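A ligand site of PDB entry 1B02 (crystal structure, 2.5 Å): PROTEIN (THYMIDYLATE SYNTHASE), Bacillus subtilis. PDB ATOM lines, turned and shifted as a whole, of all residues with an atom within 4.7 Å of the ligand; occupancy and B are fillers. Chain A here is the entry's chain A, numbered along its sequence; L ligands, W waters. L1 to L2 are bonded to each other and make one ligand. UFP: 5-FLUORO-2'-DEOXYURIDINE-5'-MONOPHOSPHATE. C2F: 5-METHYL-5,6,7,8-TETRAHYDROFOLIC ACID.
The backbone NH (N) of Cys 161 sits at hydrogen-bond distance from the side-chain hydroxyl (OH) of Tyr 108, at 3.3 Å. The backbone carbonyl oxygen of Asn 183 lies within hydrogen-bond range of the backbone NH of His 222. OD1 of Asn 192 is in hydrogen-bond range of ND2 of Asn 183 (3.0 Å). OD1 of Asn 192 lies close to O of Gly 188 (3.1 Å). The side-chain carboxylate (OD1) of Asp 184 is in hydrogen-bond range of the backbone NH (N) of Leu 187, at 3.2 Å. The backbone carbonyl oxygen of Asp 184 is in hydrogen-bond range of the backbone NH of Asn 189 (3.0 Å). The backbone carbonyl oxygen (O) of Thr 159 sits at hydrogen-bond distance from the guanidinium group (NH2) of Arg 181 (2.7 Å). ND2 of Asn 189 sits at hydrogen-bond distance from OD1 of Asn 183, at 2.8 Å.
OH of Tyr 108 sits close to F5 of UFP L1, 2.9 Å away. Residues that only touch the ligand: Ala 64 (3.6 Å), Thr 67 (3.6 Å), Ile 93 (3.3 Å), Trp 94 (3.7 Å), Trp 97 (3.2 Å), Leu 158 (3.8 Å), Val 162 (3.7 Å), Leu 187 (3.9 Å) and Leu 273 (3.8 Å). Hydrophobic or aromatic side chains that line the ligand: Ala 64, Ile 93, Trp 94, Trp 97, Leu 158, Val 162, Leu 187, His 222, Tyr 224 and Ala 278. 21 residues have an atom within 4 Å of the ligand: Arg 28, Ala 64, Thr 67, Ile 93, Trp 94, Trp 97, Tyr 108, Leu 158, Cys 161, Val 162, Arg 181, Ser 182, Asn 183, Asp 184, Leu 187, Gly 188, Asn 192, His 222, Tyr 224, Leu 273 and Ala 278. The nearest printed residue that does not touch the ligand is Phe 191 (4.01 Å).
The side-chain sulfur of Cys 161 is bonded to a carbon (C6) of UFP L1, at 1.7 Å. NE2 of His 222 lies within hydrogen-bond range of O3' of UFP L1 (2.6 Å). The side-chain amide oxygen (OD1) of Asn 192 sits at hydrogen-bond distance from a nitrogen (N3) of UFP L1 (2.7 Å). OG of Ser 182 lies within hydrogen-bond range of O2P of UFP L1, at 2.7 Å. The backbone NH of Asp 184 lies within hydrogen-bond range of an oxygen (O2) of UFP L1. The side-chain carboxylate (OD2) of Asp 184 sits at hydrogen-bond distance from a nitrogen (N3) of C2F L2, 2.8 Å away. The side-chain hydroxyl (OH) of Tyr 224 lies within hydrogen-bond range of an oxygen (O3') of UFP L1. The guanidinium group (NE) of Arg 28 lies within salt-bridge range of an oxygen (O3P) of UFP L1. NA2 of C2F L2 lies within hydrogen-bond range of O of Ala 278 (2.9 Å). An oxygen (O1P) of UFP L1 lies within salt-bridge range of the guanidinium group of Arg 181, at 2.9 Å. ND2 of Asn 183 is in hydrogen-bond range of O2 of UFP L1, 3.0 Å away. N of Gly 188 lies within hydrogen-bond range of O4 of C2F L2, at 3.1 Å.
Water W10 lies within hydrogen-bond range of N1 of C2F L2 (2.7 Å), O of Ala 278 (2.9 Å) and NH2 of Arg 28 (3.0 Å). Water W3 lies within hydrogen-bond range of an oxygen (O2) of C2F L2 (2.8 Å), the side-chain amino group (NZ) of Lys 61 (2.9 Å) and the backbone carbonyl oxygen (O) of Leu 273 (3.0 Å). Water W1 lies within hydrogen-bond range of OH of Tyr 108 (2.6 Å), O4 of UFP L1 (2.8 Å), N of Val 162 (3.1 Å) and N of Cys 161 (3.4 Å). Water W8 lies within hydrogen-bond range of NZ of Lys 61, O1 of C2F L2 and O of Leu 187. Water W4 bridges the side-chain carboxylate (OE2) of Glu 71 (2.8 Å) and a nitrogen (N10) of C2F L2 (3.5 Å).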
ATOM      1  N   ARG A  28      22.459   8.415  -2.977  1.00  0.00           N
ATOM      2  CA  ARG A  28      21.136   8.445  -2.354  1.00  0.00           C
ATOM      3  C   ARG A  28      21.122   7.975  -0.901  1.00  0.00           C
ATOM      4  O   ARG A  28      20.320   8.453  -0.091  1.00  0.00           O
ATOM      5  CB  ARG A  28      20.171   7.581  -3.165  1.00  0.00           C
ATOM      6  CG  ARG A  28      18.826   7.344  -2.493  1.00  0.00           C
ATOM      7  CD  ARG A  28      18.155   6.088  -3.023  1.00  0.00           C
ATOM      8  NE  ARG A  28      18.632   4.887  -2.348  1.00  0.00           N
ATOM      9  CZ  ARG A  28      18.280   4.519  -1.126  1.00  0.00           C
ATOM     10  NH1 ARG A  28      17.430   5.260  -0.422  1.00  0.00           N
ATOM     11  NH2 ARG A  28      18.771   3.410  -0.589  1.00  0.00           N
ATOM     12  N   THR A  29      22.014   7.056  -0.568  1.00  0.00           N
ATOM     13  CA  THR A  29      22.074   6.497   0.778  1.00  0.00           C
ATOM     14  C   THR A  29      22.830   7.328   1.820  1.00  0.00           C
ATOM     15  O   THR A  29      23.860   7.935   1.529  1.00  0.00           O
ATOM     16  CB  THR A  29      22.688   5.093   0.742  1.00  0.00           C
ATOM     17  OG1 THR A  29      23.921   5.145   0.018  1.00  0.00           O
ATOM     18  CG2 THR A  29      21.741   4.119   0.048  1.00  0.00           C
ATOM     19  N   LYS A  61      29.958 -16.436   9.013  1.00  0.00           N
ATOM     20  CA  LYS A  61      29.278 -15.542   9.948  1.00  0.00           C
ATOM     21  C   LYS A  61      27.888 -16.079  10.221  1.00  0.00           C
ATOM     22  O   LYS A  61      27.393 -16.943   9.504  1.00  0.00           O
ATOM     23  CB  LYS A  61      29.194 -14.127   9.354  1.00  0.00           C
ATOM     24  CG  LYS A  61      27.810 -13.759   8.840  1.00  0.00           C
ATOM     25  CD  LYS A  61      27.818 -12.430   8.093  1.00  0.00           C
ATOM     26  CE  LYS A  61      26.500 -12.226   7.367  1.00  0.00           C
ATOM     27  NZ  LYS A  61      26.410 -10.855   6.800  1.00  0.00           N
ATOM     28  N   ALA A  64      20.975 -14.694   9.833  1.00  0.00           N
ATOM     29  CA  ALA A  64      19.639 -14.741  10.404  1.00  0.00           C
ATOM     30  C   ALA A  64      18.689 -15.369   9.380  1.00  0.00           C
ATOM     31  O   ALA A  64      17.767 -14.715   8.891  1.00  0.00           O
ATOM     32  CB  ALA A  64      19.172 -13.331  10.759  1.00  0.00           C
ATOM     33  N   THR A  67      14.866 -15.073   9.762  1.00  0.00           N
ATOM     34  CA  THR A  67      14.356 -13.752   9.382  1.00  0.00           C
ATOM     35  C   THR A  67      14.237 -13.645   7.866  1.00  0.00           C
ATOM     36  O   THR A  67      13.275 -13.073   7.357  1.00  0.00           O
ATOM     37  CB  THR A  67      15.307 -12.642   9.875  1.00  0.00           C
ATOM     38  OG1 THR A  67      15.504 -12.787  11.288  1.00  0.00           O
ATOM     39  CG2 THR A  67      14.729 -11.272   9.591  1.00  0.00           C
ATOM     40  N   GLU A  71      10.777 -12.869   5.792  1.00  0.00           N
ATOM     41  CA  GLU A  71      10.615 -11.774   4.851  1.00  0.00           C
ATOM     42  C   GLU A  71      10.093 -12.319   3.529  1.00  0.00           C
ATOM     43  O   GLU A  71       9.211 -11.728   2.901  1.00  0.00           O
ATOM     44  CB  GLU A  71      11.948 -11.073   4.622  1.00  0.00           C
ATOM     45  CG  GLU A  71      11.894  -9.971   3.571  1.00  0.00           C
ATOM     46  CD  GLU A  71      13.275  -9.480   3.185  1.00  0.00           C
ATOM     47  OE1 GLU A  71      14.206 -10.303   3.122  1.00  0.00           O
ATOM     48  OE2 GLU A  71      13.421  -8.259   2.949  1.00  0.00           O
ATOM     49  N   ILE A  93      13.734  -5.326   9.949  1.00  0.00           N
ATOM     50  CA  ILE A  93      14.712  -4.950   8.932  1.00  0.00           C
ATOM     51  C   ILE A  93      14.165  -3.954   7.909  1.00  0.00           C
ATOM     52  O   ILE A  93      14.938  -3.350   7.164  1.00  0.00           O
ATOM     53  CB  ILE A  93      15.223  -6.199   8.178  1.00  0.00           C
ATOM     54  CG1 ILE A  93      14.046  -6.908   7.483  1.00  0.00           C
ATOM     55  CG2 ILE A  93      15.920  -7.138   9.152  1.00  0.00           C
ATOM     56  CD1 ILE A  93      14.464  -8.038   6.565  1.00  0.00           C
ATOM     57  N   TRP A  94      12.849  -3.777   7.885  1.00  0.00           N
ATOM     58  CA  TRP A  94      12.207  -2.856   6.951  1.00  0.00           C
ATOM     59  C   TRP A  94      11.634  -1.609   7.629  1.00  0.00           C
ATOM     60  O   TRP A  94      11.118  -0.717   6.972  1.00  0.00           O
ATOM     61  CB  TRP A  94      11.068  -3.574   6.194  1.00  0.00           C
ATOM     62  CG  TRP A  94      11.528  -4.276   4.959  1.00  0.00           C
ATOM     63  CD1 TRP A  94      11.848  -5.593   4.824  1.00  0.00           C
ATOM     64  CD2 TRP A  94      11.768  -3.673   3.670  1.00  0.00           C
ATOM     65  NE1 TRP A  94      12.266  -5.857   3.539  1.00  0.00           N
ATOM     66  CE2 TRP A  94      12.224  -4.696   2.816  1.00  0.00           C
ATOM     67  CE3 TRP A  94      11.636  -2.372   3.169  1.00  0.00           C
ATOM     68  CZ2 TRP A  94      12.554  -4.453   1.471  1.00  0.00           C
ATOM     69  CZ3 TRP A  94      11.962  -2.130   1.833  1.00  0.00           C
ATOM     70  CH2 TRP A  94      12.420  -3.175   0.999  1.00  0.00           C
ATOM     71  N   TRP A  97      12.191   2.126   6.414  1.00  0.00           N
ATOM     72  CA  TRP A  97      11.524   2.685   5.243  1.00  0.00           C
ATOM     73  C   TRP A  97      10.016   2.663   5.349  1.00  0.00           C
ATOM     74  O   TRP A  97       9.308   3.040   4.407  1.00  0.00           O
ATOM     75  CB  TRP A  97      11.988   1.935   3.985  1.00  0.00           C
ATOM     76  CG  TRP A  97      13.467   1.984   3.828  1.00  0.00           C
ATOM     77  CD1 TRP A  97      14.195   2.929   3.164  1.00  0.00           C
ATOM     78  CD2 TRP A  97      14.423   1.075   4.396  1.00  0.00           C
ATOM     79  NE1 TRP A  97      15.538   2.680   3.289  1.00  0.00           N
ATOM     80  CE2 TRP A  97      15.708   1.550   4.049  1.00  0.00           C
ATOM     81  CE3 TRP A  97      14.313  -0.079   5.183  1.00  0.00           C
ATOM     82  CZ2 TRP A  97      16.881   0.899   4.448  1.00  0.00           C
ATOM     83  CZ3 TRP A  97      15.479  -0.723   5.579  1.00  0.00           C
ATOM     84  CH2 TRP A  97      16.740  -0.236   5.214  1.00  0.00           C
ATOM     85  N   TYR A 108       6.890  -4.651  -3.751  1.00  0.00           N
ATOM     86  CA  TYR A 108       7.033  -6.028  -3.284  1.00  0.00           C
ATOM     87  C   TYR A 108       5.706  -6.779  -3.226  1.00  0.00           C
ATOM     88  O   TYR A 108       5.032  -6.936  -4.246  1.00  0.00           O
ATOM     89  CB  TYR A 108       7.709  -6.026  -1.912  1.00  0.00           C
ATOM     90  CG  TYR A 108       9.172  -5.662  -1.979  1.00  0.00           C
ATOM     91  CD1 TYR A 108       9.584  -4.329  -1.973  1.00  0.00           C
ATOM     92  CD2 TYR A 108      10.147  -6.657  -2.069  1.00  0.00           C
ATOM     93  CE1 TYR A 108      10.945  -3.993  -2.068  1.00  0.00           C
ATOM     94  CE2 TYR A 108      11.502  -6.329  -2.166  1.00  0.00           C
ATOM     95  CZ  TYR A 108      11.885  -4.998  -2.161  1.00  0.00           C
ATOM     96  OH  TYR A 108      13.221  -4.678  -2.266  1.00  0.00           O
ATOM     97  N   LEU A 158      10.727   2.213  -1.614  1.00  0.00           N
ATOM     98  CA  LEU A 158      12.069   1.851  -2.062  1.00  0.00           C
ATOM     99  C   LEU A 158      11.937   0.840  -3.190  1.00  0.00           C
ATOM    100  O   LEU A 158      11.431  -0.268  -2.979  1.00  0.00           O
ATOM    101  CB  LEU A 158      12.864   1.246  -0.902  1.00  0.00           C
ATOM    102  CG  LEU A 158      14.332   0.901  -1.164  1.00  0.00           C
ATOM    103  CD1 LEU A 158      15.146   1.168   0.094  1.00  0.00           C
ATOM    104  CD2 LEU A 158      14.472  -0.555  -1.586  1.00  0.00           C
ATOM    105  N   THR A 159      12.375   1.221  -4.380  1.00  0.00           N
ATOM    106  CA  THR A 159      12.304   0.330  -5.531  1.00  0.00           C
ATOM    107  C   THR A 159      13.027  -0.973  -5.201  1.00  0.00           C
ATOM    108  O   THR A 159      14.098  -0.972  -4.603  1.00  0.00           O
ATOM    109  CB  THR A 159      12.920   0.997  -6.766  1.00  0.00           C
ATOM    110  OG1 THR A 159      14.271   1.367  -6.489  1.00  0.00           O
ATOM    111  CG2 THR A 159      12.125   2.238  -7.137  1.00  0.00           C
ATOM    112  N   CYS A 161      15.216  -4.332  -4.932  1.00  0.00           N
ATOM    113  CA  CYS A 161      16.611  -4.624  -5.250  1.00  0.00           C
ATOM    114  C   CYS A 161      16.637  -5.910  -6.074  1.00  0.00           C
ATOM    115  O   CYS A 161      17.254  -5.974  -7.135  1.00  0.00           O
ATOM    116  CB  CYS A 161      17.417  -4.799  -3.971  1.00  0.00           C
ATOM    117  SG  CYS A 161      17.199  -3.458  -2.754  1.00  0.00           S
ATOM    118  N   VAL A 162      15.960  -6.937  -5.557  1.00  0.00           N
ATOM    119  CA  VAL A 162      15.817  -8.214  -6.250  1.00  0.00           C
ATOM    120  C   VAL A 162      14.403  -8.083  -6.781  1.00  0.00           C
ATOM    121  O   VAL A 162      13.431  -8.374  -6.086  1.00  0.00           O
ATOM    122  CB  VAL A 162      15.923  -9.408  -5.282  1.00  0.00           C
ATOM    123  CG1 VAL A 162      15.857 -10.718  -6.056  1.00  0.00           C
ATOM    124  CG2 VAL A 162      17.218  -9.332  -4.503  1.00  0.00           C
ATOM    125  N   ARG A 181      19.200  -5.715  -9.111  1.00  0.00           N
ATOM    126  CA  ARG A 181      19.715  -4.539  -9.793  1.00  0.00           C
ATOM    127  C   ARG A 181      20.779  -3.867  -8.928  1.00  0.00           C
ATOM    128  O   ARG A 181      21.739  -3.285  -9.437  1.00  0.00           O
ATOM    129  CB  ARG A 181      18.585  -3.542 -10.067  1.00  0.00           C
ATOM    130  CG  ARG A 181      17.880  -3.073  -8.819  1.00  0.00           C
ATOM    131  CD  ARG A 181      17.338  -1.664  -8.960  1.00  0.00           C
ATOM    132  NE  ARG A 181      16.634  -1.251  -7.747  1.00  0.00           N
ATOM    133  CZ  ARG A 181      17.208  -0.611  -6.730  1.00  0.00           C
ATOM    134  NH1 ARG A 181      18.498  -0.297  -6.788  1.00  0.00           N
ATOM    135  NH2 ARG A 181      16.503  -0.278  -5.661  1.00  0.00           N
ATOM    136  N   SER A 182      20.596  -3.976  -7.617  1.00  0.00           N
ATOM    137  CA  SER A 182      21.493  -3.401  -6.627  1.00  0.00           C
ATOM    138  C   SER A 182      21.637  -4.386  -5.471  1.00  0.00           C
ATOM    139  O   SER A 182      20.636  -4.872  -4.949  1.00  0.00           O
ATOM    140  CB  SER A 182      20.915  -2.077  -6.116  1.00  0.00           C
ATOM    141  OG  SER A 182      21.854  -1.370  -5.325  1.00  0.00           O
ATOM    142  N   ASN A 183      22.875  -4.676  -5.068  1.00  0.00           N
ATOM    143  CA  ASN A 183      23.087  -5.624  -3.981  1.00  0.00           C
ATOM    144  C   ASN A 183      24.101  -5.177  -2.936  1.00  0.00           C
ATOM    145  O   ASN A 183      25.276  -4.947  -3.244  1.00  0.00           O
ATOM    146  CB  ASN A 183      23.524  -6.979  -4.535  1.00  0.00           C
ATOM    147  CG  ASN A 183      22.704  -8.134  -3.972  1.00  0.00           C
ATOM    148  OD1 ASN A 183      23.155  -9.276  -3.962  1.00  0.00           O
ATOM    149  ND2 ASN A 183      21.491  -7.840  -3.514  1.00  0.00           N
ATOM    150  N   ASP A 184      23.632  -5.058  -1.691  1.00  0.00           N
ATOM    151  CA  ASP A 184      24.478  -4.685  -0.542  1.00  0.00           C
ATOM    152  C   ASP A 184      25.074  -6.016  -0.110  1.00  0.00           C
ATOM    153  O   ASP A 184      24.443  -6.792   0.611  1.00  0.00           O
ATOM    154  CB  ASP A 184      23.596  -4.091   0.567  1.00  0.00           C
ATOM    155  CG  ASP A 184      24.340  -3.882   1.881  1.00  0.00           C
ATOM    156  OD1 ASP A 184      25.489  -4.369   2.026  1.00  0.00           O
ATOM    157  OD2 ASP A 184      23.760  -3.226   2.772  1.00  0.00           O
ATOM    158  N   LEU A 187      24.985  -6.870   3.920  1.00  0.00           N
ATOM    159  CA  LEU A 187      23.673  -7.128   4.507  1.00  0.00           C
ATOM    160  C   LEU A 187      22.692  -7.921   3.642  1.00  0.00           C
ATOM    161  O   LEU A 187      22.386  -9.072   3.932  1.00  0.00           O
ATOM    162  CB  LEU A 187      23.032  -5.799   4.921  1.00  0.00           C
ATOM    163  CG  LEU A 187      23.103  -5.353   6.383  1.00  0.00           C
ATOM    164  CD1 LEU A 187      24.098  -6.196   7.162  1.00  0.00           C
ATOM    165  CD2 LEU A 187      23.497  -3.888   6.434  1.00  0.00           C
ATOM    166  N   GLY A 188      22.198  -7.288   2.581  1.00  0.00           N
ATOM    167  CA  GLY A 188      21.221  -7.924   1.718  1.00  0.00           C
ATOM    168  C   GLY A 188      21.575  -9.224   1.011  1.00  0.00           C
ATOM    169  O   GLY A 188      20.799 -10.169   1.040  1.00  0.00           O
ATOM    170  N   ASN A 189      22.735  -9.273   0.359  1.00  0.00           N
ATOM    171  CA  ASN A 189      23.121 -10.470  -0.372  1.00  0.00           C
ATOM    172  C   ASN A 189      22.958 -11.790   0.363  1.00  0.00           C
ATOM    173  O   ASN A 189      22.267 -12.687  -0.118  1.00  0.00           O
ATOM    174  CB  ASN A 189      24.553 -10.346  -0.892  1.00  0.00           C
ATOM    175  CG  ASN A 189      24.962 -11.528  -1.753  1.00  0.00           C
ATOM    176  OD1 ASN A 189      25.795 -12.341  -1.360  1.00  0.00           O
ATOM    177  ND2 ASN A 189      24.359 -11.631  -2.935  1.00  0.00           N
ATOM    178  N   PHE A 191      21.145 -12.561   2.650  1.00  0.00           N
ATOM    179  CA  PHE A 191      19.709 -12.736   2.836  1.00  0.00           C
ATOM    180  C   PHE A 191      19.045 -13.144   1.525  1.00  0.00           C
ATOM    181  O   PHE A 191      18.256 -14.081   1.486  1.00  0.00           O
ATOM    182  CB  PHE A 191      19.073 -11.429   3.304  1.00  0.00           C
ATOM    183  CG  PHE A 191      18.806 -11.360   4.789  1.00  0.00           C
ATOM    184  CD1 PHE A 191      19.796 -11.697   5.696  1.00  0.00           C
ATOM    185  CD2 PHE A 191      17.572 -10.919   5.259  1.00  0.00           C
ATOM    186  CE1 PHE A 191      19.568 -11.592   7.069  1.00  0.00           C
ATOM    187  CE2 PHE A 191      17.324 -10.822   6.625  1.00  0.00           C
ATOM    188  CZ  PHE A 191      18.327 -11.159   7.537  1.00  0.00           C
ATOM    189  N   ASN A 192      19.377 -12.429   0.459  1.00  0.00           N
ATOM    190  CA  ASN A 192      18.806 -12.666  -0.870  1.00  0.00           C
ATOM    191  C   ASN A 192      19.111 -14.030  -1.472  1.00  0.00           C
ATOM    192  O   ASN A 192      18.197 -14.750  -1.871  1.00  0.00           O
ATOM    193  CB  ASN A 192      19.281 -11.580  -1.839  1.00  0.00           C
ATOM    194  CG  ASN A 192      18.865 -10.183  -1.413  1.00  0.00           C
ATOM    195  OD1 ASN A 192      19.598  -9.220  -1.617  1.00  0.00           O
ATOM    196  ND2 ASN A 192      17.680 -10.062  -0.830  1.00  0.00           N
ATOM    197  N   HIS A 222      27.969  -3.881  -4.875  1.00  0.00           N
ATOM    198  CA  HIS A 222      28.769  -3.003  -4.027  1.00  0.00           C
ATOM    199  C   HIS A 222      28.978  -3.426  -2.575  1.00  0.00           C
ATOM    200  O   HIS A 222      28.366  -4.376  -2.083  1.00  0.00           O
ATOM    201  CB  HIS A 222      28.127  -1.614  -4.035  1.00  0.00           C
ATOM    202  CG  HIS A 222      26.685  -1.621  -3.638  1.00  0.00           C
ATOM    203  ND1 HIS A 222      25.665  -1.726  -4.544  1.00  0.00           N
ATOM    204  CD2 HIS A 222      26.106  -1.539  -2.413  1.00  0.00           C
ATOM    205  CE1 HIS A 222      24.505  -1.712  -3.906  1.00  0.00           C
ATOM    206  NE2 HIS A 222      24.748  -1.600  -2.607  1.00  0.00           N
ATOM    207  N   TYR A 224      29.552  -1.157   1.077  1.00  0.00           N
ATOM    208  CA  TYR A 224      29.664   0.140   1.749  1.00  0.00           C
ATOM    209  C   TYR A 224      30.983   0.282   2.510  1.00  0.00           C
ATOM    210  O   TYR A 224      31.436  -0.664   3.162  1.00  0.00           O
ATOM    211  CB  TYR A 224      28.474   0.353   2.678  1.00  0.00           C
ATOM    212  CG  TYR A 224      27.173   0.602   1.940  1.00  0.00           C
ATOM    213  CD1 TYR A 224      26.796   1.891   1.573  1.00  0.00           C
ATOM    214  CD2 TYR A 224      26.319  -0.457   1.603  1.00  0.00           C
ATOM    215  CE1 TYR A 224      25.598   2.132   0.883  1.00  0.00           C
ATOM    216  CE2 TYR A 224      25.120  -0.231   0.921  1.00  0.00           C
ATOM    217  CZ  TYR A 224      24.769   1.061   0.564  1.00  0.00           C
ATOM    218  OH  TYR A 224      23.595   1.303  -0.107  1.00  0.00           O
ATOM    219  N   LEU A 273      28.381 -10.771  12.988  1.00  0.00           N
ATOM    220  CA  LEU A 273      29.134  -9.587  12.605  1.00  0.00           C
ATOM    221  C   LEU A 273      28.160  -8.417  12.431  1.00  0.00           C
ATOM    222  O   LEU A 273      27.114  -8.564  11.810  1.00  0.00           O
ATOM    223  CB  LEU A 273      29.876  -9.843  11.278  1.00  0.00           C
ATOM    224  CG  LEU A 273      31.398 -10.016  11.270  1.00  0.00           C
ATOM    225  CD1 LEU A 273      31.959  -9.989  12.687  1.00  0.00           C
ATOM    226  CD2 LEU A 273      31.745 -11.316  10.581  1.00  0.00           C
ATOM    227  N   VAL A 277      23.487  -0.162   8.645  1.00  0.00           N
ATOM    228  CA  VAL A 277      22.640  -0.108   7.460  1.00  0.00           C
ATOM    229  C   VAL A 277      22.523   1.304   6.876  1.00  0.00           C
ATOM    230  O   VAL A 277      22.297   2.266   7.606  1.00  0.00           O
ATOM    231  CB  VAL A 277      21.216  -0.676   7.750  1.00  0.00           C
ATOM    232  CG1 VAL A 277      21.117  -1.103   9.198  1.00  0.00           C
ATOM    233  CG2 VAL A 277      20.135   0.341   7.421  1.00  0.00           C
ATOM    234  N   ALA A 278      22.690   1.398   5.569  1.00  0.00           N
ATOM    235  CA  ALA A 278      22.579   2.672   4.871  1.00  0.00           C
ATOM    236  C   ALA A 278      21.128   2.791   4.422  1.00  0.00           C
ATOM    237  O   ALA A 278      20.603   1.885   3.777  1.00  0.00           O
ATOM    238  CB  ALA A 278      23.514   2.697   3.665  1.00  0.00           C
HETATM  239  N1  UFP L   1      19.460  -4.197  -1.247  1.00  0.00           N
HETATM  240  C2  UFP L   1      19.902  -5.533  -1.382  1.00  0.00           C
HETATM  241  N3  UFP L   1      18.971  -6.619  -1.355  1.00  0.00           N
HETATM  242  C4  UFP L   1      17.555  -6.520  -1.047  1.00  0.00           C
HETATM  243  C5  UFP L   1      16.945  -5.102  -0.466  1.00  0.00           C
HETATM  244  C6  UFP L   1      17.866  -3.924  -1.247  1.00  0.00           C
HETATM  245  O2  UFP L   1      21.087  -5.881  -1.257  1.00  0.00           O
HETATM  246  O4  UFP L   1      16.758  -7.412  -1.342  1.00  0.00           O
HETATM  247  F5  UFP L   1      15.643  -4.941  -0.625  1.00  0.00           F
HETATM  248  C1' UFP L   1      20.397  -3.025  -1.117  1.00  0.00           C
HETATM  249  C2' UFP L   1      21.211  -2.633  -2.331  1.00  0.00           C
HETATM  250  C3' UFP L   1      21.460  -1.179  -1.961  1.00  0.00           C
HETATM  251  C4' UFP L   1      20.250  -0.697  -1.213  1.00  0.00           C
HETATM  252  O3' UFP L   1      22.607  -1.102  -1.149  1.00  0.00           O
HETATM  253  O4' UFP L   1      19.691  -1.860  -0.620  1.00  0.00           O
HETATM  254  C5' UFP L   1      19.090   0.031  -1.931  1.00  0.00           C
HETATM  255  O5' UFP L   1      19.611   1.313  -2.401  1.00  0.00           O
HETATM  256  P   UFP L   1      19.505   1.670  -3.937  1.00  0.00           P
HETATM  257  O1P UFP L   1      18.065   1.769  -4.246  1.00  0.00           O
HETATM  258  O2P UFP L   1      20.304   0.735  -4.694  1.00  0.00           O
HETATM  259  O3P UFP L   1      20.313   3.028  -3.926  1.00  0.00           O
HETATM  260  N1  C2F L   2      19.345  -1.006   2.615  1.00  0.00           N
HETATM  261  C2  C2F L   2      20.693  -1.468   2.727  1.00  0.00           C
HETATM  262  NA2 C2F L   2      21.774  -0.578   2.761  1.00  0.00           N
HETATM  263  N3  C2F L   2      21.006  -2.828   2.576  1.00  0.00           N
HETATM  264  C4  C2F L   2      19.956  -3.823   2.396  1.00  0.00           C
HETATM  265  O4  C2F L   2      20.183  -5.016   2.162  1.00  0.00           O
HETATM  266  C4A C2F L   2      18.542  -3.279   2.202  1.00  0.00           C
HETATM  267  N5  C2F L   2      17.354  -4.160   2.088  1.00  0.00           N
HETATM  268  C6  C2F L   2      16.104  -3.735   2.562  1.00  0.00           C
HETATM  269  C7  C2F L   2      15.811  -2.315   2.128  1.00  0.00           C
HETATM  270  N8  C2F L   2      16.984  -1.412   2.218  1.00  0.00           N
HETATM  271  C8A C2F L   2      18.303  -1.887   2.244  1.00  0.00           C
HETATM  272  C9  C2F L   2      15.880  -3.905   4.099  1.00  0.00           C
HETATM  273  N10 C2F L   2      16.393  -5.303   4.422  1.00  0.00           N
HETATM  274  C11 C2F L   2      17.287  -5.286   1.135  1.00  0.00           C
HETATM  275  C12 C2F L   2      19.327  -6.098   7.509  1.00  0.00           C
HETATM  276  C13 C2F L   2      18.899  -4.759   7.234  1.00  0.00           C
HETATM  277  C14 C2F L   2      17.988  -4.467   6.203  1.00  0.00           C
HETATM  278  C15 C2F L   2      17.530  -5.514   5.316  1.00  0.00           C
HETATM  279  C16 C2F L   2      18.072  -6.847   5.505  1.00  0.00           C
HETATM  280  C17 C2F L   2      18.892  -7.134   6.579  1.00  0.00           C
HETATM  281  C   C2F L   2      20.156  -6.461   8.740  1.00  0.00           C
HETATM  282  O   C2F L   2      20.348  -5.549   9.596  1.00  0.00           O
HETATM  283  N   C2F L   2      20.698  -7.781   8.781  1.00  0.00           N
HETATM  284  CA  C2F L   2      21.283  -8.125  10.096  1.00  0.00           C
HETATM  285  CB  C2F L   2      20.254  -9.033  10.814  1.00  0.00           C
HETATM  286  CG  C2F L   2      19.915  -9.254  12.306  1.00  0.00           C
HETATM  287  CD  C2F L   2      18.364  -9.494  12.446  1.00  0.00           C
HETATM  288  OE1 C2F L   2      17.662  -8.430  12.437  1.00  0.00           O
HETATM  289  OE2 C2F L   2      18.004 -10.638  12.802  1.00  0.00           O
HETATM  290  CT  C2F L   2      22.630  -8.777   9.812  1.00  0.00           C
HETATM  291  O1  C2F L   2      22.559  -9.650   8.906  1.00  0.00           O
HETATM  292  O2  C2F L   2      23.593  -8.398  10.493  1.00  0.00           O
HETATM  293  O   HOH W   1      14.401  -6.938  -2.827  1.00  0.00           O
HETATM  294  O   HOH W   2      16.469  -5.446  12.607  1.00  0.00           O
HETATM  295  O   HOH W   3      25.763  -9.738   9.381  1.00  0.00           O
HETATM  296  O   HOH W   4      16.229  -8.196   2.514  1.00  0.00           O
HETATM  297  O   HOH W   5      20.579   4.607  -6.172  1.00  0.00           O
HETATM  298  O   HOH W   6      18.066  -3.676  10.108  1.00  0.00           O
HETATM  299  O   HOH W   7      14.504  -8.028  12.586  1.00  0.00           O
HETATM  300  O   HOH W   8      23.845 -10.333   6.393  1.00  0.00           O
HETATM  301  O   HOH W   9      22.677  -4.626  10.709  1.00  0.00           O
HETATM  302  O   HOH W  10      18.603   1.453   1.708  1.00  0.00           O
